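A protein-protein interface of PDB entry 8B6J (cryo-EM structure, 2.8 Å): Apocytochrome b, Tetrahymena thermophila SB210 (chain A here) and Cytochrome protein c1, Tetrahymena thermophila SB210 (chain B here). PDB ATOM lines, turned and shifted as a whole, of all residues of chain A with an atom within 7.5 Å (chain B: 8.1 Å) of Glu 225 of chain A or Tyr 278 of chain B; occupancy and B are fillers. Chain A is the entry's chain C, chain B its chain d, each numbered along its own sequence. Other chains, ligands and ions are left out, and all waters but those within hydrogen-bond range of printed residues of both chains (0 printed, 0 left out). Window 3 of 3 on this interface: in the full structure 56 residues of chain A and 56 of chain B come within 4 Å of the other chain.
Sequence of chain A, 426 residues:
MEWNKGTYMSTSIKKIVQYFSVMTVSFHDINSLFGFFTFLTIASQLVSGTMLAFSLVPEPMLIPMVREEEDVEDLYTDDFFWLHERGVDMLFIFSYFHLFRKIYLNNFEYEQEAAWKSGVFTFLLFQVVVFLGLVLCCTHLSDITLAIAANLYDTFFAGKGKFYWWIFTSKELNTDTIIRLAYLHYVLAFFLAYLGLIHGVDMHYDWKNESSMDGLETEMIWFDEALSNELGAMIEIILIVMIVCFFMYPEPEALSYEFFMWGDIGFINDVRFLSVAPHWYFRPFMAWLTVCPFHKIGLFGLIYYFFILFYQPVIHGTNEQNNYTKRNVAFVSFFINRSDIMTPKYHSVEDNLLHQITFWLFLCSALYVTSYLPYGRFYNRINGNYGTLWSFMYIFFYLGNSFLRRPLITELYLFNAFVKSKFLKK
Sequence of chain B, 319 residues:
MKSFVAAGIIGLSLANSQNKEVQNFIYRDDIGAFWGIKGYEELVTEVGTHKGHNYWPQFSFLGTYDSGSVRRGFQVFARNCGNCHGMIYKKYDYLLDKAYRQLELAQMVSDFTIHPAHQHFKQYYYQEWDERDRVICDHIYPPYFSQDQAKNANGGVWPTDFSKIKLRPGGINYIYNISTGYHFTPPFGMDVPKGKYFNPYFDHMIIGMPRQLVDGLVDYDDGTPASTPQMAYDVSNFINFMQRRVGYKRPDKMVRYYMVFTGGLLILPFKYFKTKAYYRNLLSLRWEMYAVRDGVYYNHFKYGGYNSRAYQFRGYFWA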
ATOM      1  N   VAL A  25     -34.683 -28.642  25.491  1.00  0.00           N
ATOM      2  CA  VAL A  25     -34.761 -29.501  26.665  1.00  0.00           C
ATOM      3  C   VAL A  25     -34.280 -28.710  27.872  1.00  0.00           C
ATOM      4  O   VAL A  25     -33.188 -28.130  27.846  1.00  0.00           O
ATOM      5  CB  VAL A  25     -33.923 -30.780  26.487  1.00  0.00           C
ATOM      6  CG1 VAL A  25     -34.093 -31.696  27.686  1.00  0.00           C
ATOM      7  CG2 VAL A  25     -34.310 -31.493  25.203  1.00  0.00           C
ATOM      8  N   PHE A  27     -32.768 -28.137  31.629  1.00  0.00           N
ATOM      9  CA  PHE A  27     -31.649 -28.784  32.299  1.00  0.00           C
ATOM     10  C   PHE A  27     -32.148 -29.918  33.187  1.00  0.00           C
ATOM     11  O   PHE A  27     -33.135 -29.771  33.913  1.00  0.00           O
ATOM     12  CB  PHE A  27     -30.866 -27.760  33.118  1.00  0.00           C
ATOM     13  CG  PHE A  27     -30.270 -26.662  32.286  1.00  0.00           C
ATOM     14  CD1 PHE A  27     -29.049 -26.835  31.662  1.00  0.00           C
ATOM     15  CD2 PHE A  27     -30.935 -25.461  32.121  1.00  0.00           C
ATOM     16  CE1 PHE A  27     -28.502 -25.831  30.893  1.00  0.00           C
ATOM     17  CE2 PHE A  27     -30.392 -24.453  31.354  1.00  0.00           C
ATOM     18  CZ  PHE A  27     -29.174 -24.639  30.739  1.00  0.00           C
ATOM     19  N   HIS A  28     -31.459 -31.055  33.121  1.00  0.00           N
ATOM     20  CA  HIS A  28     -31.953 -32.295  33.699  1.00  0.00           C
ATOM     21  C   HIS A  28     -30.798 -33.068  34.322  1.00  0.00           C
ATOM     22  O   HIS A  28     -29.654 -32.606  34.355  1.00  0.00           O
ATOM     23  CB  HIS A  28     -32.661 -33.134  32.633  1.00  0.00           C
ATOM     24  CG  HIS A  28     -31.828 -33.382  31.415  1.00  0.00           C
ATOM     25  ND1 HIS A  28     -31.727 -32.473  30.385  1.00  0.00           N
ATOM     26  CD2 HIS A  28     -31.052 -34.434  31.065  1.00  0.00           C
ATOM     27  CE1 HIS A  28     -30.929 -32.956  29.450  1.00  0.00           C
ATOM     28  NE2 HIS A  28     -30.506 -34.144  29.839  1.00  0.00           N
ATOM     29  N   GLU A 219     -33.376 -22.957  28.019  1.00  0.00           N
ATOM     30  CA  GLU A 219     -33.330 -24.396  27.814  1.00  0.00           C
ATOM     31  C   GLU A 219     -32.224 -24.724  26.824  1.00  0.00           C
ATOM     32  O   GLU A 219     -31.763 -23.867  26.067  1.00  0.00           O
ATOM     33  CB  GLU A 219     -34.672 -24.933  27.302  1.00  0.00           C
ATOM     34  CG  GLU A 219     -35.846 -24.663  28.226  1.00  0.00           C
ATOM     35  CD  GLU A 219     -37.161 -25.141  27.647  1.00  0.00           C
ATOM     36  OE1 GLU A 219     -37.191 -25.495  26.450  1.00  0.00           O
ATOM     37  OE2 GLU A 219     -38.166 -25.162  28.389  1.00  0.00           O
ATOM     38  N   MET A 220     -31.801 -25.982  26.845  1.00  0.00           N
ATOM     39  CA  MET A 220     -30.808 -26.472  25.904  1.00  0.00           C
ATOM     40  C   MET A 220     -31.455 -26.755  24.553  1.00  0.00           C
ATOM     41  O   MET A 220     -32.678 -26.858  24.429  1.00  0.00           O
ATOM     42  CB  MET A 220     -30.154 -27.746  26.434  1.00  0.00           C
ATOM     43  CG  MET A 220     -29.484 -27.593  27.785  1.00  0.00           C
ATOM     44  SD  MET A 220     -29.660 -29.069  28.805  1.00  0.00           S
ATOM     45  CE  MET A 220     -29.163 -30.339  27.650  1.00  0.00           C
ATOM     46  N   ILE A 221     -30.617 -26.874  23.530  1.00  0.00           N
ATOM     47  CA  ILE A 221     -31.057 -27.337  22.220  1.00  0.00           C
ATOM     48  C   ILE A 221     -30.838 -28.840  22.160  1.00  0.00           C
ATOM     49  O   ILE A 221     -29.756 -29.333  22.501  1.00  0.00           O
ATOM     50  CB  ILE A 221     -30.303 -26.613  21.091  1.00  0.00           C
ATOM     51  CG1 ILE A 221     -30.993 -26.850  19.745  1.00  0.00           C
ATOM     52  CG2 ILE A 221     -28.863 -27.082  21.019  1.00  0.00           C
ATOM     53  CD1 ILE A 221     -32.344 -26.182  19.621  1.00  0.00           C
ATOM     54  N   TRP A 222     -31.867 -29.577  21.743  1.00  0.00           N
ATOM     55  CA  TRP A 222     -31.822 -31.029  21.880  1.00  0.00           C
ATOM     56  C   TRP A 222     -30.728 -31.651  21.023  1.00  0.00           C
ATOM     57  O   TRP A 222     -30.058 -32.594  21.459  1.00  0.00           O
ATOM     58  CB  TRP A 222     -33.171 -31.646  21.518  1.00  0.00           C
ATOM     59  CG  TRP A 222     -33.127 -33.143  21.543  1.00  0.00           C
ATOM     60  CD1 TRP A 222     -33.271 -33.946  22.633  1.00  0.00           C
ATOM     61  CD2 TRP A 222     -32.907 -34.016  20.428  1.00  0.00           C
ATOM     62  NE1 TRP A 222     -33.159 -35.264  22.269  1.00  0.00           N
ATOM     63  CE2 TRP A 222     -32.936 -35.334  20.919  1.00  0.00           C
ATOM     64  CE3 TRP A 222     -32.691 -33.810  19.063  1.00  0.00           C
ATOM     65  CZ2 TRP A 222     -32.757 -36.441  20.094  1.00  0.00           C
ATOM     66  CZ3 TRP A 222     -32.513 -34.910  18.246  1.00  0.00           C
ATOM     67  CH2 TRP A 222     -32.548 -36.209  18.764  1.00  0.00           C
ATOM     68  N   PHE A 223     -30.529 -31.148  19.803  1.00  0.00           N
ATOM     69  CA  PHE A 223     -29.776 -31.909  18.810  1.00  0.00           C
ATOM     70  C   PHE A 223     -28.403 -32.322  19.324  1.00  0.00           C
ATOM     71  O   PHE A 223     -27.990 -33.474  19.155  1.00  0.00           O
ATOM     72  CB  PHE A 223     -29.621 -31.112  17.518  1.00  0.00           C
ATOM     73  CG  PHE A 223     -28.633 -31.723  16.567  1.00  0.00           C
ATOM     74  CD1 PHE A 223     -28.721 -33.063  16.229  1.00  0.00           C
ATOM     75  CD2 PHE A 223     -27.611 -30.968  16.024  1.00  0.00           C
ATOM     76  CE1 PHE A 223     -27.814 -33.634  15.367  1.00  0.00           C
ATOM     77  CE2 PHE A 223     -26.703 -31.537  15.157  1.00  0.00           C
ATOM     78  CZ  PHE A 223     -26.806 -32.872  14.829  1.00  0.00           C
ATOM     79  N   ASP A 224     -27.674 -31.397  19.935  1.00  0.00           N
ATOM     80  CA  ASP A 224     -26.315 -31.681  20.378  1.00  0.00           C
ATOM     81  C   ASP A 224     -26.119 -31.507  21.874  1.00  0.00           C
ATOM     82  O   ASP A 224     -25.434 -32.321  22.496  1.00  0.00           O
ATOM     83  CB  ASP A 224     -25.324 -30.780  19.634  1.00  0.00           C
ATOM     84  CG  ASP A 224     -23.909 -31.321  19.670  1.00  0.00           C
ATOM     85  OD1 ASP A 224     -23.613 -32.162  20.542  1.00  0.00           O
ATOM     86  OD2 ASP A 224     -23.089 -30.901  18.826  1.00  0.00           O
ATOM     87  N   GLU A 225     -26.700 -30.468  22.472  1.00  0.00           N
ATOM     88  CA  GLU A 225     -26.496 -30.239  23.898  1.00  0.00           C
ATOM     89  C   GLU A 225     -27.147 -31.336  24.730  1.00  0.00           C
ATOM     90  O   GLU A 225     -26.518 -31.899  25.633  1.00  0.00           O
ATOM     91  CB  GLU A 225     -27.039 -28.866  24.288  1.00  0.00           C
ATOM     92  CG  GLU A 225     -26.338 -27.719  23.585  1.00  0.00           C
ATOM     93  CD  GLU A 225     -26.919 -26.370  23.945  1.00  0.00           C
ATOM     94  OE1 GLU A 225     -27.833 -26.318  24.794  1.00  0.00           O
ATOM     95  OE2 GLU A 225     -26.461 -25.359  23.375  1.00  0.00           O
ATOM     96  N   ALA A 226     -28.408 -31.660  24.438  1.00  0.00           N
ATOM     97  CA  ALA A 226     -29.091 -32.708  25.188  1.00  0.00           C
ATOM     98  C   ALA A 226     -28.742 -34.093  24.659  1.00  0.00           C
ATOM     99  O   ALA A 226     -28.625 -35.045  25.437  1.00  0.00           O
ATOM    100  CB  ALA A 226     -30.603 -32.492  25.140  1.00  0.00           C
ATOM    101  N   LEU A 227     -28.585 -34.226  23.341  1.00  0.00           N
ATOM    102  CA  LEU A 227     -28.271 -35.529  22.763  1.00  0.00           C
ATOM    103  C   LEU A 227     -26.925 -36.041  23.255  1.00  0.00           C
ATOM    104  O   LEU A 227     -26.783 -37.227  23.577  1.00  0.00           O
ATOM    105  CB  LEU A 227     -28.278 -35.437  21.239  1.00  0.00           C
ATOM    106  CG  LEU A 227     -28.008 -36.736  20.476  1.00  0.00           C
ATOM    107  CD1 LEU A 227     -29.107 -37.752  20.732  1.00  0.00           C
ATOM    108  CD2 LEU A 227     -27.867 -36.457  18.992  1.00  0.00           C
ATOM    109  N   SER A 228     -25.919 -35.167  23.302  1.00  0.00           N
ATOM    110  CA  SER A 228     -24.605 -35.588  23.772  1.00  0.00           C
ATOM    111  C   SER A 228     -24.664 -36.038  25.224  1.00  0.00           C
ATOM    112  O   SER A 228     -24.069 -37.058  25.591  1.00  0.00           O
ATOM    113  CB  SER A 228     -23.600 -34.449  23.599  1.00  0.00           C
ATOM    114  OG  SER A 228     -24.010 -33.298  24.314  1.00  0.00           O
ATOM    115  N   ASN A 229     -25.383 -35.292  26.064  1.00  0.00           N
ATOM    116  CA  ASN A 229     -25.521 -35.681  27.462  1.00  0.00           C
ATOM    117  C   ASN A 229     -26.236 -37.018  27.592  1.00  0.00           C
ATOM    118  O   ASN A 229     -25.850 -37.858  28.411  1.00  0.00           O
ATOM    119  CB  ASN A 229     -26.272 -34.598  28.235  1.00  0.00           C
ATOM    120  CG  ASN A 229     -26.572 -35.004  29.662  1.00  0.00           C
ATOM    121  OD1 ASN A 229     -25.900 -35.862  30.231  1.00  0.00           O
ATOM    122  ND2 ASN A 229     -27.590 -34.388  30.249  1.00  0.00           N
ATOM    123  N   GLU A 230     -27.287 -37.231  26.800  1.00  0.00           N
ATOM    124  CA  GLU A 230     -28.012 -38.494  26.863  1.00  0.00           C
ATOM    125  C   GLU A 230     -27.128 -39.661  26.441  1.00  0.00           C
ATOM    126  O   GLU A 230     -27.122 -40.713  27.092  1.00  0.00           O
ATOM    127  CB  GLU A 230     -29.262 -38.413  25.989  1.00  0.00           C
ATOM    128  CG  GLU A 230     -30.308 -37.448  26.519  1.00  0.00           C
ATOM    129  CD  GLU A 230     -31.385 -37.131  25.503  1.00  0.00           C
ATOM    130  OE1 GLU A 230     -31.224 -37.512  24.326  1.00  0.00           O
ATOM    131  OE2 GLU A 230     -32.394 -36.499  25.882  1.00  0.00           O
ATOM    132  N   LYS B 271     -17.037 -36.326  28.171  1.00  0.00           N
ATOM    133  CA  LYS B 271     -18.471 -36.176  28.389  1.00  0.00           C
ATOM    134  C   LYS B 271     -18.745 -35.134  29.463  1.00  0.00           C
ATOM    135  O   LYS B 271     -19.646 -34.299  29.315  1.00  0.00           O
ATOM    136  CB  LYS B 271     -19.089 -37.516  28.788  1.00  0.00           C
ATOM    137  CG  LYS B 271     -20.578 -37.439  29.114  1.00  0.00           C
ATOM    138  CD  LYS B 271     -21.004 -38.540  30.067  1.00  0.00           C
ATOM    139  CE  LYS B 271     -22.406 -38.289  30.604  1.00  0.00           C
ATOM    140  NZ  LYS B 271     -22.476 -37.074  31.460  1.00  0.00           N
ATOM    141  N   TYR B 272     -17.994 -35.183  30.564  1.00  0.00           N
ATOM    142  CA  TYR B 272     -18.180 -34.196  31.619  1.00  0.00           C
ATOM    143  C   TYR B 272     -17.990 -32.788  31.074  1.00  0.00           C
ATOM    144  O   TYR B 272     -18.852 -31.919  31.249  1.00  0.00           O
ATOM    145  CB  TYR B 272     -17.211 -34.464  32.770  1.00  0.00           C
ATOM    146  CG  TYR B 272     -17.448 -33.582  33.972  1.00  0.00           C
ATOM    147  CD1 TYR B 272     -16.870 -32.325  34.061  1.00  0.00           C
ATOM    148  CD2 TYR B 272     -18.257 -34.005  35.015  1.00  0.00           C
ATOM    149  CE1 TYR B 272     -17.089 -31.516  35.156  1.00  0.00           C
ATOM    150  CE2 TYR B 272     -18.481 -33.204  36.112  1.00  0.00           C
ATOM    151  CZ  TYR B 272     -17.894 -31.959  36.178  1.00  0.00           C
ATOM    152  OH  TYR B 272     -18.115 -31.157  37.273  1.00  0.00           O
ATOM    153  N   PHE B 273     -16.877 -32.561  30.375  1.00  0.00           N
ATOM    154  CA  PHE B 273     -16.610 -31.243  29.806  1.00  0.00           C
ATOM    155  C   PHE B 273     -17.738 -30.807  28.884  1.00  0.00           C
ATOM    156  O   PHE B 273     -18.197 -29.661  28.941  1.00  0.00           O
ATOM    157  CB  PHE B 273     -15.287 -31.259  29.038  1.00  0.00           C
ATOM    158  CG  PHE B 273     -14.080 -31.483  29.899  1.00  0.00           C
ATOM    159  CD1 PHE B 273     -13.947 -30.838  31.116  1.00  0.00           C
ATOM    160  CD2 PHE B 273     -13.075 -32.337  29.487  1.00  0.00           C
ATOM    161  CE1 PHE B 273     -12.835 -31.045  31.902  1.00  0.00           C
ATOM    162  CE2 PHE B 273     -11.965 -32.548  30.269  1.00  0.00           C
ATOM    163  CZ  PHE B 273     -11.842 -31.901  31.479  1.00  0.00           C
ATOM    164  N   LYS B 274     -18.197 -31.710  28.019  1.00  0.00           N
ATOM    165  CA  LYS B 274     -19.163 -31.345  26.994  1.00  0.00           C
ATOM    166  C   LYS B 274     -20.569 -31.153  27.542  1.00  0.00           C
ATOM    167  O   LYS B 274     -21.374 -30.474  26.898  1.00  0.00           O
ATOM    168  CB  LYS B 274     -19.182 -32.412  25.899  1.00  0.00           C
ATOM    169  CG  LYS B 274     -20.112 -32.116  24.737  1.00  0.00           C
ATOM    170  CD  LYS B 274     -19.766 -30.803  24.062  1.00  0.00           C
ATOM    171  CE  LYS B 274     -20.481 -30.666  22.732  1.00  0.00           C
ATOM    172  NZ  LYS B 274     -21.959 -30.752  22.875  1.00  0.00           N
ATOM    173  N   THR B 275     -20.891 -31.728  28.701  1.00  0.00           N
ATOM    174  CA  THR B 275     -22.252 -31.666  29.217  1.00  0.00           C
ATOM    175  C   THR B 275     -22.369 -30.839  30.492  1.00  0.00           C
ATOM    176  O   THR B 275     -23.043 -29.807  30.497  1.00  0.00           O
ATOM    177  CB  THR B 275     -22.769 -33.088  29.475  1.00  0.00           C
ATOM    178  OG1 THR B 275     -22.014 -33.687  30.534  1.00  0.00           O
ATOM    179  CG2 THR B 275     -22.646 -33.946  28.223  1.00  0.00           C
ATOM    180  N   LYS B 276     -21.666 -31.215  31.559  1.00  0.00           N
ATOM    181  CA  LYS B 276     -21.999 -30.661  32.868  1.00  0.00           C
ATOM    182  C   LYS B 276     -21.316 -29.320  33.097  1.00  0.00           C
ATOM    183  O   LYS B 276     -21.959 -28.351  33.520  1.00  0.00           O
ATOM    184  CB  LYS B 276     -21.629 -31.662  33.962  1.00  0.00           C
ATOM    185  CG  LYS B 276     -22.263 -33.020  33.736  1.00  0.00           C
ATOM    186  CD  LYS B 276     -22.400 -33.822  35.011  1.00  0.00           C
ATOM    187  CE  LYS B 276     -23.212 -35.080  34.755  1.00  0.00           C
ATOM    188  NZ  LYS B 276     -23.384 -35.908  35.975  1.00  0.00           N
ATOM    189  N   ALA B 277     -20.015 -29.243  32.825  1.00  0.00           N
ATOM    190  CA  ALA B 277     -19.342 -27.953  32.880  1.00  0.00           C
ATOM    191  C   ALA B 277     -19.960 -26.983  31.885  1.00  0.00           C
ATOM    192  O   ALA B 277     -20.063 -25.783  32.156  1.00  0.00           O
ATOM    193  CB  ALA B 277     -17.851 -28.129  32.607  1.00  0.00           C
ATOM    194  N   TYR B 278     -20.390 -27.489  30.727  1.00  0.00           N
ATOM    195  CA  TYR B 278     -21.036 -26.631  29.740  1.00  0.00           C
ATOM    196  C   TYR B 278     -22.359 -26.082  30.262  1.00  0.00           C
ATOM    197  O   TYR B 278     -22.646 -24.890  30.102  1.00  0.00           O
ATOM    198  CB  TYR B 278     -21.247 -27.404  28.440  1.00  0.00           C
ATOM    199  CG  TYR B 278     -21.933 -26.604  27.360  1.00  0.00           C
ATOM    200  CD1 TYR B 278     -21.323 -25.489  26.803  1.00  0.00           C
ATOM    201  CD2 TYR B 278     -23.186 -26.966  26.890  1.00  0.00           C
ATOM    202  CE1 TYR B 278     -21.946 -24.756  25.816  1.00  0.00           C
ATOM    203  CE2 TYR B 278     -23.814 -26.238  25.902  1.00  0.00           C
ATOM    204  CZ  TYR B 278     -23.190 -25.135  25.369  1.00  0.00           C
ATOM    205  OH  TYR B 278     -23.813 -24.407  24.383  1.00  0.00           O
ATOM    206  N   TYR B 279     -23.180 -26.930  30.889  1.00  0.00           N
ATOM    207  CA  TYR B 279     -24.423 -26.439  31.476  1.00  0.00           C
ATOM    208  C   TYR B 279     -24.140 -25.409  32.559  1.00  0.00           C
ATOM    209  O   TYR B 279     -24.821 -24.382  32.643  1.00  0.00           O
ATOM    210  CB  TYR B 279     -25.236 -27.598  32.051  1.00  0.00           C
ATOM    211  CG  TYR B 279     -25.610 -28.664  31.048  1.00  0.00           C
ATOM    212  CD1 TYR B 279     -25.643 -28.392  29.689  1.00  0.00           C
ATOM    213  CD2 TYR B 279     -25.927 -29.950  31.466  1.00  0.00           C
ATOM    214  CE1 TYR B 279     -25.981 -29.369  28.774  1.00  0.00           C
ATOM    215  CE2 TYR B 279     -26.266 -30.932  30.559  1.00  0.00           C
ATOM    216  CZ  TYR B 279     -26.292 -30.637  29.216  1.00  0.00           C
ATOM    217  OH  TYR B 279     -26.629 -31.613  28.309  1.00  0.00           O
ATOM    218  N   ARG B 280     -23.138 -25.668  33.401  1.00  0.00           N
ATOM    219  CA  ARG B 280     -22.786 -24.702  34.435  1.00  0.00           C
ATOM    220  C   ARG B 280     -22.355 -23.376  33.818  1.00  0.00           C
ATOM    221  O   ARG B 280     -22.656 -22.304  34.354  1.00  0.00           O
ATOM    222  CB  ARG B 280     -21.685 -25.271  35.332  1.00  0.00           C
ATOM    223  CG  ARG B 280     -21.215 -24.318  36.414  1.00  0.00           C
ATOM    224  CD  ARG B 280     -20.664 -25.055  37.629  1.00  0.00           C
ATOM    225  NE  ARG B 280     -19.631 -26.027  37.284  1.00  0.00           N
ATOM    226  CZ  ARG B 280     -19.820 -27.337  37.185  1.00  0.00           C
ATOM    227  NH1 ARG B 280     -21.007 -27.885  37.392  1.00  0.00           N
ATOM    228  NH2 ARG B 280     -18.792 -28.119  36.874  1.00  0.00           N
ATOM    229  N   ASN B 281     -21.646 -23.430  32.688  1.00  0.00           N
ATOM    230  CA  ASN B 281     -21.281 -22.205  31.983  1.00  0.00           C
ATOM    231  C   ASN B 281     -22.515 -21.478  31.464  1.00  0.00           C
ATOM    232  O   ASN B 281     -22.602 -20.249  31.553  1.00  0.00           O
ATOM    233  CB  ASN B 281     -20.332 -22.524  30.828  1.00  0.00           C
ATOM    234  CG  ASN B 281     -18.929 -22.845  31.296  1.00  0.00           C
ATOM    235  OD1 ASN B 281     -18.506 -22.413  32.367  1.00  0.00           O
ATOM    236  ND2 ASN B 281     -18.197 -23.601  30.489  1.00  0.00           N
ATOM    237  N   LEU B 282     -23.476 -22.221  30.909  1.00  0.00           N
ATOM    238  CA  LEU B 282     -24.667 -21.584  30.354  1.00  0.00           C
ATOM    239  C   LEU B 282     -25.540 -20.968  31.438  1.00  0.00           C
ATOM    240  O   LEU B 282     -26.275 -20.013  31.169  1.00  0.00           O
ATOM    241  CB  LEU B 282     -25.480 -22.595  29.546  1.00  0.00           C
ATOM    242  CG  LEU B 282     -24.915 -23.025  28.191  1.00  0.00           C
ATOM    243  CD1 LEU B 282     -25.857 -24.014  27.530  1.00  0.00           C
ATOM    244  CD2 LEU B 282     -24.678 -21.828  27.284  1.00  0.00           C
ATOM    245  N   LEU B 283     -25.478 -21.494  32.658  1.00  0.00           N
ATOM    246  CA  LEU B 283     -26.308 -21.007  33.752  1.00  0.00           C
ATOM    247  C   LEU B 283     -25.745 -19.759  34.417  1.00  0.00           C
ATOM    248  O   LEU B 283     -26.402 -19.205  35.305  1.00  0.00           O
ATOM    249  CB  LEU B 283     -26.489 -22.110  34.795  1.00  0.00           C
ATOM    250  CG  LEU B 283     -27.290 -23.322  34.319  1.00  0.00           C
ATOM    251  CD1 LEU B 283     -27.091 -24.496  35.257  1.00  0.00           C
ATOM    252  CD2 LEU B 283     -28.764 -22.973  34.207  1.00  0.00           C
ATOM    253  N   SER B 284     -24.556 -19.307  34.020  1.00  0.00           N
ATOM    254  CA  SER B 284     -23.946 -18.107  34.592  1.00  0.00           C
ATOM    255  C   SER B 284     -24.647 -16.887  34.001  1.00  0.00           C
ATOM    256  O   SER B 284     -24.159 -16.223  33.083  1.00  0.00           O
ATOM    257  CB  SER B 284     -22.450 -18.085  34.317  1.00  0.00           C
ATOM    258  OG  SER B 284     -21.837 -19.286  34.751  1.00  0.00           O
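Among the printed residues, merely in contact across the chains: Met 220 of chain A with Tyr 279 of chain B (2.9 Å), Asn 229 of chain A with Tyr 279 of chain B (3.0 Å), Asn 229 of chain A with Thr 275 of chain B (3.4 Å), Ser 228 of chain A with Lys 274 of chain B (3.6 Å), Phe 27 of chain A with Leu 283 of chain B (3.6 Å), Asn 229 of chain A with Lys 271 of chain B (3.8 Å) and Phe 27 of chain A with Tyr 279 of chain B (3.9 Å).
Of the 14 printed residues of chain B, 6 touch a printed residue of chain A.
Among the printed residues, 10 pairs touch across the chains.
Glu 225 of chain A touches just these residues of chain B: Tyr 278 and Tyr 279.
Tyr 278 of chain B touches one residue of chain A.
No residue of chain B comes within 4 Å of Ala 226 of chain A.
Of the printed residues of chain B, Asn 229 of chain A touches Lys 271, Thr 275 and Tyr 279.
Of the printed residues of chain A, Thr 275 of chain B touches Asn 229 (3.4 Å).
Printed residues of chain B within 4 Å of Ser 228 of chain A: Lys 274 (3.6 Å).
Glu 230 of chain A touches none of the printed residues of chain B.
Lys 276 of chain B touches none of the printed residues of chain A.
The nearest residue of chain B that does not touch Glu 225 of chain A is Leu 282 of chain B (4.1 Å).
The nearest printed residue of chain A that does not touch Thr 275 of chain B is Ser 228 of chain A (4.2 Å).
The side-chain hydroxyl (OH) of Tyr 279 of chain B sits at hydrogen-bond distance from the backbone carbonyl oxygen (O) of Glu 225 of chain A (2.7 Å).
OH of Tyr 278 of chain B sits at hydrogen-bond distance from OE2 of Glu 225 of chain A (3.0 Å).
NZ of Lys 274 of chain B lies within salt-bridge range of OD1 of Asp 224 of chain A.
The backbone carbonyl oxygen (O) of Asp 224 of chain A is in hydrogen-bond range of the side-chain hydroxyl (OG) of Ser 228 of chain A (2.5 Å).
A ring nitrogen (NE2) of His 28 of chain A sits at hydrogen-bond distance from the side-chain amide nitrogen of Asn 229 of chain A (3.0 Å).
N of Ile 221 of chain A lies within hydrogen-bond range of OE1 of Glu 225 of chain A, at 3.1 Å.
The backbone carbonyl oxygen of Glu 225 of chain A sits at hydrogen-bond distance from the side-chain hydroxyl of Ser 228 of chain A (3.2 Å).
OG1 of Thr 275 of chain B is in hydrogen-bond range of O of Lys 271 of chain B (2.7 Å).
The backbone carbonyl oxygen of Val 25 of chain A lies within hydrogen-bond range of the backbone NH of Met 220 of chain A.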
